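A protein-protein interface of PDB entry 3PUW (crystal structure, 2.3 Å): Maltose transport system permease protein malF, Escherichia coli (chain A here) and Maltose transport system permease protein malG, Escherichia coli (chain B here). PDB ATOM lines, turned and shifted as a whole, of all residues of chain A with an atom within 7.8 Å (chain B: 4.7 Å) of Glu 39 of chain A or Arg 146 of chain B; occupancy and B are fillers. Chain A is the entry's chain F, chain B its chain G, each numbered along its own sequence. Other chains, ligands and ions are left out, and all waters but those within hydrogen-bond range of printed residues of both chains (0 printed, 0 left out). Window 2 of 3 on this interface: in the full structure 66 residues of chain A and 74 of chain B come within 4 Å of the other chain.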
ATOM      1  N   LEU A  30     -11.896 -11.279   0.489  1.00  0.00           N
ATOM      2  CA  LEU A  30     -12.121 -10.070  -0.297  1.00  0.00           C
ATOM      3  C   LEU A  30     -13.396 -10.157  -1.137  1.00  0.00           C
ATOM      4  O   LEU A  30     -14.037  -9.139  -1.385  1.00  0.00           O
ATOM      5  CB  LEU A  30     -10.913  -9.761  -1.190  1.00  0.00           C
ATOM      6  CG  LEU A  30      -9.668  -9.141  -0.543  1.00  0.00           C
ATOM      7  CD1 LEU A  30      -8.471  -9.234  -1.477  1.00  0.00           C
ATOM      8  CD2 LEU A  30      -9.905  -7.690  -0.132  1.00  0.00           C
ATOM      9  N   VAL A  31     -13.760 -11.367  -1.560  1.00  0.00           N
ATOM     10  CA  VAL A  31     -14.924 -11.580  -2.429  1.00  0.00           C
ATOM     11  C   VAL A  31     -16.252 -11.343  -1.706  1.00  0.00           C
ATOM     12  O   VAL A  31     -17.099 -10.594  -2.195  1.00  0.00           O
ATOM     13  CB  VAL A  31     -14.903 -12.983  -3.094  1.00  0.00           C
ATOM     14  CG1 VAL A  31     -16.201 -13.253  -3.855  1.00  0.00           C
ATOM     15  CG2 VAL A  31     -13.709 -13.112  -4.027  1.00  0.00           C
ATOM     16  N   LEU A  33     -16.508  -9.821   1.101  1.00  0.00           N
ATOM     17  CA  LEU A  33     -16.378  -8.440   1.562  1.00  0.00           C
ATOM     18  C   LEU A  33     -16.771  -7.448   0.461  1.00  0.00           C
ATOM     19  O   LEU A  33     -17.291  -6.369   0.750  1.00  0.00           O
ATOM     20  CB  LEU A  33     -14.949  -8.188   2.062  1.00  0.00           C
ATOM     21  CG  LEU A  33     -14.517  -6.946   2.859  1.00  0.00           C
ATOM     22  CD1 LEU A  33     -13.913  -5.893   1.948  1.00  0.00           C
ATOM     23  CD2 LEU A  33     -15.626  -6.347   3.734  1.00  0.00           C
ATOM     24  N   MET A  34     -16.521  -7.824  -0.793  1.00  0.00           N
ATOM     25  CA  MET A  34     -16.987  -7.054  -1.951  1.00  0.00           C
ATOM     26  C   MET A  34     -18.489  -7.238  -2.164  1.00  0.00           C
ATOM     27  O   MET A  34     -19.166  -6.329  -2.650  1.00  0.00           O
ATOM     28  CB  MET A  34     -16.234  -7.458  -3.221  1.00  0.00           C
ATOM     29  CG  MET A  34     -14.852  -6.837  -3.367  1.00  0.00           C
ATOM     30  SD  MET A  34     -13.884  -7.612  -4.680  1.00  0.00           S
ATOM     31  CE  MET A  34     -12.307  -6.786  -4.467  1.00  0.00           C
ATOM     32  N   TYR A  35     -18.997  -8.415  -1.799  1.00  0.00           N
ATOM     33  CA  TYR A  35     -20.421  -8.735  -1.921  1.00  0.00           C
ATOM     34  C   TYR A  35     -21.277  -7.826  -1.035  1.00  0.00           C
ATOM     35  O   TYR A  35     -22.423  -7.525  -1.371  1.00  0.00           O
ATOM     36  CB  TYR A  35     -20.670 -10.208  -1.579  1.00  0.00           C
ATOM     37  CG  TYR A  35     -22.030 -10.728  -1.995  1.00  0.00           C
ATOM     38  CD1 TYR A  35     -22.241 -11.237  -3.278  1.00  0.00           C
ATOM     39  CD2 TYR A  35     -23.104 -10.721  -1.105  1.00  0.00           C
ATOM     40  CE1 TYR A  35     -23.490 -11.719  -3.666  1.00  0.00           C
ATOM     41  CE2 TYR A  35     -24.356 -11.198  -1.483  1.00  0.00           C
ATOM     42  CZ  TYR A  35     -24.541 -11.696  -2.763  1.00  0.00           C
ATOM     43  OH  TYR A  35     -25.778 -12.169  -3.138  1.00  0.00           O
ATOM     44  N   ALA A  36     -20.704  -7.394   0.087  1.00  0.00           N
ATOM     45  CA  ALA A  36     -21.357  -6.452   0.996  1.00  0.00           C
ATOM     46  C   ALA A  36     -21.349  -5.024   0.436  1.00  0.00           C
ATOM     47  O   ALA A  36     -20.848  -4.788  -0.666  1.00  0.00           O
ATOM     48  CB  ALA A  36     -20.696  -6.500   2.371  1.00  0.00           C
ATOM     49  N   GLN A  37     -21.894  -4.088   1.215  1.00  0.00           N
ATOM     50  CA  GLN A  37     -22.097  -2.670   0.832  1.00  0.00           C
ATOM     51  C   GLN A  37     -22.752  -2.410  -0.540  1.00  0.00           C
ATOM     52  O   GLN A  37     -23.758  -1.697  -0.618  1.00  0.00           O
ATOM     53  CB  GLN A  37     -20.838  -1.796   1.058  1.00  0.00           C
ATOM     54  CG  GLN A  37     -19.626  -2.065   0.156  1.00  0.00           C
ATOM     55  CD  GLN A  37     -18.513  -2.828   0.856  1.00  0.00           C
ATOM     56  OE1 GLN A  37     -18.748  -3.845   1.510  1.00  0.00           O
ATOM     57  NE2 GLN A  37     -17.287  -2.340   0.712  1.00  0.00           N
ATOM     58  N   GLY A  38     -22.184  -2.980  -1.603  1.00  0.00           N
ATOM     59  CA  GLY A  38     -22.748  -2.872  -2.947  1.00  0.00           C
ATOM     60  C   GLY A  38     -21.710  -2.827  -4.052  1.00  0.00           C
ATOM     61  O   GLY A  38     -21.543  -1.796  -4.710  1.00  0.00           O
ATOM     62  N   GLU A  39     -21.014  -3.945  -4.254  1.00  0.00           N
ATOM     63  CA  GLU A  39     -20.003  -4.071  -5.310  1.00  0.00           C
ATOM     64  C   GLU A  39     -20.119  -5.426  -6.012  1.00  0.00           C
ATOM     65  O   GLU A  39     -19.216  -6.262  -5.925  1.00  0.00           O
ATOM     66  CB  GLU A  39     -18.588  -3.880  -4.741  1.00  0.00           C
ATOM     67  CG  GLU A  39     -18.223  -2.442  -4.375  1.00  0.00           C
ATOM     68  CD  GLU A  39     -18.110  -1.525  -5.584  1.00  0.00           C
ATOM     69  OE1 GLU A  39     -17.693  -1.995  -6.666  1.00  0.00           O
ATOM     70  OE2 GLU A  39     -18.435  -0.327  -5.447  1.00  0.00           O
ATOM     71  N   TYR A  40     -21.232  -5.626  -6.713  1.00  0.00           N
ATOM     72  CA  TYR A  40     -21.566  -6.926  -7.305  1.00  0.00           C
ATOM     73  C   TYR A  40     -20.744  -7.270  -8.550  1.00  0.00           C
ATOM     74  O   TYR A  40     -20.161  -8.355  -8.632  1.00  0.00           O
ATOM     75  CB  TYR A  40     -23.068  -7.011  -7.607  1.00  0.00           C
ATOM     76  CG  TYR A  40     -23.949  -6.805  -6.394  1.00  0.00           C
ATOM     77  CD1 TYR A  40     -24.570  -5.579  -6.161  1.00  0.00           C
ATOM     78  CD2 TYR A  40     -24.160  -7.834  -5.476  1.00  0.00           C
ATOM     79  CE1 TYR A  40     -25.381  -5.382  -5.047  1.00  0.00           C
ATOM     80  CE2 TYR A  40     -24.969  -7.649  -4.358  1.00  0.00           C
ATOM     81  CZ  TYR A  40     -25.576  -6.421  -4.150  1.00  0.00           C
ATOM     82  OH  TYR A  40     -26.375  -6.231  -3.048  1.00  0.00           O
ATOM     83  N   LEU A  41     -20.698  -6.344  -9.507  1.00  0.00           N
ATOM     84  CA  LEU A  41     -19.937  -6.528 -10.743  1.00  0.00           C
ATOM     85  C   LEU A  41     -18.464  -6.800 -10.447  1.00  0.00           C
ATOM     86  O   LEU A  41     -17.821  -7.585 -11.145  1.00  0.00           O
ATOM     87  CB  LEU A  41     -20.083  -5.299 -11.653  1.00  0.00           C
ATOM     88  CG  LEU A  41     -19.746  -5.407 -13.148  1.00  0.00           C
ATOM     89  CD1 LEU A  41     -20.617  -4.454 -13.958  1.00  0.00           C
ATOM     90  CD2 LEU A  41     -18.268  -5.154 -13.435  1.00  0.00           C
ATOM     91  N   PHE A  42     -17.944  -6.157  -9.405  1.00  0.00           N
ATOM     92  CA  PHE A  42     -16.548  -6.321  -9.014  1.00  0.00           C
ATOM     93  C   PHE A  42     -16.302  -7.640  -8.284  1.00  0.00           C
ATOM     94  O   PHE A  42     -15.190  -8.158  -8.302  1.00  0.00           O
ATOM     95  CB  PHE A  42     -16.081  -5.143  -8.153  1.00  0.00           C
ATOM     96  CG  PHE A  42     -14.630  -4.794  -8.343  1.00  0.00           C
ATOM     97  CD1 PHE A  42     -13.637  -5.462  -7.630  1.00  0.00           C
ATOM     98  CD2 PHE A  42     -14.255  -3.797  -9.241  1.00  0.00           C
ATOM     99  CE1 PHE A  42     -12.293  -5.145  -7.807  1.00  0.00           C
ATOM    100  CE2 PHE A  42     -12.914  -3.471  -9.424  1.00  0.00           C
ATOM    101  CZ  PHE A  42     -11.931  -4.147  -8.705  1.00  0.00           C
ATOM    102  N   ALA A  43     -17.340  -8.174  -7.647  1.00  0.00           N
ATOM    103  CA  ALA A  43     -17.234  -9.440  -6.921  1.00  0.00           C
ATOM    104  C   ALA A  43     -17.291 -10.645  -7.858  1.00  0.00           C
ATOM    105  O   ALA A  43     -16.622 -11.653  -7.622  1.00  0.00           O
ATOM    106  CB  ALA A  43     -18.320  -9.537  -5.861  1.00  0.00           C
ATOM    107  N   ILE A  44     -18.097 -10.535  -8.912  1.00  0.00           N
ATOM    108  CA  ILE A  44     -18.245 -11.603  -9.903  1.00  0.00           C
ATOM    109  C   ILE A  44     -16.992 -11.689 -10.773  1.00  0.00           C
ATOM    110  O   ILE A  44     -16.490 -12.785 -11.043  1.00  0.00           O
ATOM    111  CB  ILE A  44     -19.514 -11.406 -10.783  1.00  0.00           C
ATOM    112  CG1 ILE A  44     -20.779 -11.452  -9.916  1.00  0.00           C
ATOM    113  CG2 ILE A  44     -19.585 -12.458 -11.894  1.00  0.00           C
ATOM    114  CD1 ILE A  44     -22.022 -10.864 -10.574  1.00  0.00           C
ATOM    115  N   THR A  45     -16.487 -10.530 -11.193  1.00  0.00           N
ATOM    116  CA  THR A  45     -15.301 -10.465 -12.046  1.00  0.00           C
ATOM    117  C   THR A  45     -14.039 -10.975 -11.333  1.00  0.00           C
ATOM    118  O   THR A  45     -13.228 -11.682 -11.934  1.00  0.00           O
ATOM    119  CB  THR A  45     -15.089  -9.044 -12.662  1.00  0.00           C
ATOM    120  OG1 THR A  45     -14.164  -9.119 -13.752  1.00  0.00           O
ATOM    121  CG2 THR A  45     -14.570  -8.045 -11.635  1.00  0.00           C
ATOM    122  N   THR A  46     -13.895 -10.631 -10.053  1.00  0.00           N
ATOM    123  CA  THR A  46     -12.724 -11.024  -9.268  1.00  0.00           C
ATOM    124  C   THR A  46     -12.754 -12.512  -8.908  1.00  0.00           C
ATOM    125  O   THR A  46     -11.706 -13.129  -8.696  1.00  0.00           O
ATOM    126  CB  THR A  46     -12.556 -10.151  -7.994  1.00  0.00           C
ATOM    127  OG1 THR A  46     -11.230 -10.298  -7.480  1.00  0.00           O
ATOM    128  CG2 THR A  46     -13.549 -10.544  -6.911  1.00  0.00           C
ATOM    129  N   PHE A  81     -11.418  -4.756 -20.481  1.00  0.00           N
ATOM    130  CA  PHE A  81     -12.445  -4.116 -19.659  1.00  0.00           C
ATOM    131  C   PHE A  81     -12.795  -2.699 -20.150  1.00  0.00           C
ATOM    132  O   PHE A  81     -13.976  -2.384 -20.295  1.00  0.00           O
ATOM    133  CB  PHE A  81     -12.061  -4.153 -18.170  1.00  0.00           C
ATOM    134  CG  PHE A  81     -12.802  -3.160 -17.314  1.00  0.00           C
ATOM    135  CD1 PHE A  81     -14.140  -3.361 -16.981  1.00  0.00           C
ATOM    136  CD2 PHE A  81     -12.152  -2.030 -16.821  1.00  0.00           C
ATOM    137  CE1 PHE A  81     -14.825  -2.439 -16.182  1.00  0.00           C
ATOM    138  CE2 PHE A  81     -12.828  -1.100 -16.021  1.00  0.00           C
ATOM    139  CZ  PHE A  81     -14.164  -1.307 -15.702  1.00  0.00           C
ATOM    140  N   ALA B 142     -12.950   4.523 -12.793  1.00  0.00           N
ATOM    141  CA  ALA B 142     -13.901   3.685 -12.070  1.00  0.00           C
ATOM    142  C   ALA B 142     -13.232   2.419 -11.534  1.00  0.00           C
ATOM    143  O   ALA B 142     -13.553   1.961 -10.438  1.00  0.00           O
ATOM    144  CB  ALA B 142     -15.083   3.328 -12.968  1.00  0.00           C
ATOM    145  N   LEU B 143     -12.292   1.871 -12.300  1.00  0.00           N
ATOM    146  CA  LEU B 143     -11.574   0.669 -11.887  1.00  0.00           C
ATOM    147  C   LEU B 143     -10.668   0.911 -10.681  1.00  0.00           C
ATOM    148  O   LEU B 143     -10.702   0.149  -9.717  1.00  0.00           O
ATOM    149  CB  LEU B 143     -10.779   0.067 -13.057  1.00  0.00           C
ATOM    150  CG  LEU B 143      -9.983  -1.211 -12.766  1.00  0.00           C
ATOM    151  CD1 LEU B 143     -10.913  -2.326 -12.318  1.00  0.00           C
ATOM    152  CD2 LEU B 143      -9.168  -1.643 -13.976  1.00  0.00           C
ATOM    153  N   PHE B 144      -9.868   1.970 -10.733  1.00  0.00           N
ATOM    154  CA  PHE B 144      -8.913   2.244  -9.662  1.00  0.00           C
ATOM    155  C   PHE B 144      -9.546   2.888  -8.435  1.00  0.00           C
ATOM    156  O   PHE B 144      -9.016   2.779  -7.327  1.00  0.00           O
ATOM    157  CB  PHE B 144      -7.752   3.089 -10.173  1.00  0.00           C
ATOM    158  CG  PHE B 144      -6.746   2.306 -10.951  1.00  0.00           C
ATOM    159  CD1 PHE B 144      -6.756   2.324 -12.343  1.00  0.00           C
ATOM    160  CD2 PHE B 144      -5.786   1.545 -10.294  1.00  0.00           C
ATOM    161  CE1 PHE B 144      -5.817   1.590 -13.067  1.00  0.00           C
ATOM    162  CE2 PHE B 144      -4.849   0.812 -11.007  1.00  0.00           C
ATOM    163  CZ  PHE B 144      -4.864   0.834 -12.392  1.00  0.00           C
ATOM    164  N   ASP B 145     -10.678   3.553  -8.637  1.00  0.00           N
ATOM    165  CA  ASP B 145     -11.453   4.093  -7.530  1.00  0.00           C
ATOM    166  C   ASP B 145     -11.945   2.926  -6.677  1.00  0.00           C
ATOM    167  O   ASP B 145     -11.839   2.951  -5.448  1.00  0.00           O
ATOM    168  CB  ASP B 145     -12.630   4.917  -8.057  1.00  0.00           C
ATOM    169  CG  ASP B 145     -13.297   5.750  -6.980  1.00  0.00           C
ATOM    170  OD1 ASP B 145     -12.777   5.814  -5.844  1.00  0.00           O
ATOM    171  OD2 ASP B 145     -14.350   6.351  -7.280  1.00  0.00           O
ATOM    172  N   ARG B 146     -12.460   1.902  -7.353  1.00  0.00           N
ATOM    173  CA  ARG B 146     -12.976   0.709  -6.702  1.00  0.00           C
ATOM    174  C   ARG B 146     -11.865  -0.149  -6.103  1.00  0.00           C
ATOM    175  O   ARG B 146     -12.022  -0.693  -5.013  1.00  0.00           O
ATOM    176  CB  ARG B 146     -13.819  -0.115  -7.684  1.00  0.00           C
ATOM    177  CG  ARG B 146     -15.323   0.111  -7.567  1.00  0.00           C
ATOM    178  CD  ARG B 146     -15.851   1.232  -8.466  1.00  0.00           C
ATOM    179  NE  ARG B 146     -17.122   1.768  -7.965  1.00  0.00           N
ATOM    180  CZ  ARG B 146     -18.131   2.186  -8.726  1.00  0.00           C
ATOM    181  NH1 ARG B 146     -18.055   2.123 -10.051  1.00  0.00           N
ATOM    182  NH2 ARG B 146     -19.234   2.657  -8.158  1.00  0.00           N
ATOM    183  N   LEU B 147     -10.747  -0.259  -6.811  1.00  0.00           N
ATOM    184  CA  LEU B 147      -9.628  -1.088  -6.366  1.00  0.00           C
ATOM    185  C   LEU B 147      -8.971  -0.543  -5.096  1.00  0.00           C
ATOM    186  O   LEU B 147      -8.545  -1.310  -4.229  1.00  0.00           O
ATOM    187  CB  LEU B 147      -8.590  -1.221  -7.483  1.00  0.00           C
ATOM    188  CG  LEU B 147      -7.607  -2.392  -7.439  1.00  0.00           C
ATOM    189  CD1 LEU B 147      -8.285  -3.705  -7.805  1.00  0.00           C
ATOM    190  CD2 LEU B 147      -6.444  -2.116  -8.381  1.00  0.00           C
ATOM    191  N   GLY B 148      -8.914   0.784  -4.995  1.00  0.00           N
ATOM    192  CA  GLY B 148      -8.227   1.468  -3.898  1.00  0.00           C
ATOM    193  C   GLY B 148      -8.721   1.147  -2.500  1.00  0.00           C
ATOM    194  O   GLY B 148      -7.934   1.096  -1.554  1.00  0.00           O
ATOM    195  N   GLU B 149     -10.025   0.925  -2.366  1.00  0.00           N
ATOM    196  CA  GLU B 149     -10.624   0.639  -1.063  1.00  0.00           C
ATOM    197  C   GLU B 149     -10.393  -0.797  -0.582  1.00  0.00           C
ATOM    198  O   GLU B 149     -10.810  -1.159   0.519  1.00  0.00           O
ATOM    199  CB  GLU B 149     -12.115   0.999  -1.057  1.00  0.00           C
ATOM    200  CG  GLU B 149     -12.893   0.519  -2.274  1.00  0.00           C
ATOM    201  CD  GLU B 149     -14.170   1.311  -2.512  1.00  0.00           C
ATOM    202  OE1 GLU B 149     -14.164   2.547  -2.308  1.00  0.00           O
ATOM    203  OE2 GLU B 149     -15.181   0.695  -2.915  1.00  0.00           O
ATOM    204  N   TYR B 150      -9.718  -1.603  -1.402  1.00  0.00           N
ATOM    205  CA  TYR B 150      -9.360  -2.970  -1.025  1.00  0.00           C
ATOM    206  C   TYR B 150      -7.838  -3.159  -0.969  1.00  0.00           C
ATOM    207  O   TYR B 150      -7.311  -3.685   0.013  1.00  0.00           O
ATOM    208  CB  TYR B 150     -10.040  -3.989  -1.952  1.00  0.00           C
ATOM    209  CG  TYR B 150     -11.548  -3.812  -2.029  1.00  0.00           C
ATOM    210  CD1 TYR B 150     -12.145  -3.231  -3.147  1.00  0.00           C
ATOM    211  CD2 TYR B 150     -12.373  -4.205  -0.974  1.00  0.00           C
ATOM    212  CE1 TYR B 150     -13.531  -3.054  -3.219  1.00  0.00           C
ATOM    213  CE2 TYR B 150     -13.758  -4.030  -1.035  1.00  0.00           C
ATOM    214  CZ  TYR B 150     -14.331  -3.455  -2.159  1.00  0.00           C
ATOM    215  OH  TYR B 150     -15.701  -3.285  -2.216  1.00  0.00           O
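Of the 9 printed residues of chain B, 4 touch a printed residue of chain A. Hydrophobic or aromatic side chains of chain B that line the printed part of chain A: Leu 143, Leu 147 and Tyr 150. Of the 17 printed residues of chain A, 6 touch a printed residue of chain B. Printed residues of chain A that touch a printed residue of chain B: Leu 33, Met 34, Gln 37, Glu 39, Phe 42 and Phe 81. Hydrophobic or aromatic side chains of chain A within 4 Å of the printed part of chain B: Leu 33, Met 34, Phe 42 and Phe 81. Among the printed residues, Asp or Glu carboxylates within 4 Å of a Lys or Arg side-chain nitrogen of the other chain: Glu 39 of chain A with Arg 146 of chain B.
OH of Tyr 150 of chain B sits at hydrogen-bond distance from NE2 of Gln 37 of chain A (3.5 Å). The guanidinium group (NE) of Arg 146 of chain B lies within salt-bridge range of the side-chain carboxylate (OE2) of Glu 39 of chain A.
Of chain B, only Arg 146 and Tyr 150 come within 4 Å of Glu 39 of chain A. Arg 146 of chain B touches just these residues of chain A: Glu 39 (3.3 Å) and Phe 42 (3.9 Å). Of the printed residues of chain B, Met 34 of chain A touches Tyr 150. Printed residues of chain B within 4 Å of Leu 33 of chain A: Tyr 150 (3.5 Å). Of the printed residues of chain A, Leu 143 of chain B touches Phe 42 (3.7 Å) and Phe 81 (3.8 Å). Val 31 of chain A touches none of the printed residues of chain B. The nearest printed residue of chain A that does not touch Leu 147 of chain B is Met 34 of chain A (6.1 Å).
OE1 of Gln 37 of chain A sits close to O of Leu 33 of chain A (3.0 Å). O of Met 34 of chain A sits close to N of Glu 39 of chain A (3.4 Å).
Tyr 150 of chain B touches Leu 33 of chain A (CE2 to CD1, 3.5 Å). Met 34 of chain A touches Tyr 150 of chain B. Tyr 150 of chain B touches Glu 39 of chain A (OH to CG, 3.4 Å). Phe 42 of chain A touches Leu 143 of chain B. Phe 42 of chain A touches Arg 146 of chain B (CE2 to CB, 3.9 Å). CZ of Phe 42 of chain A touches CD1 of Leu 147 of chain B, at 3.8 Å. Phe 81 of chain A touches Leu 143 of chain B (CE2 to CB, 3.8 Å).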
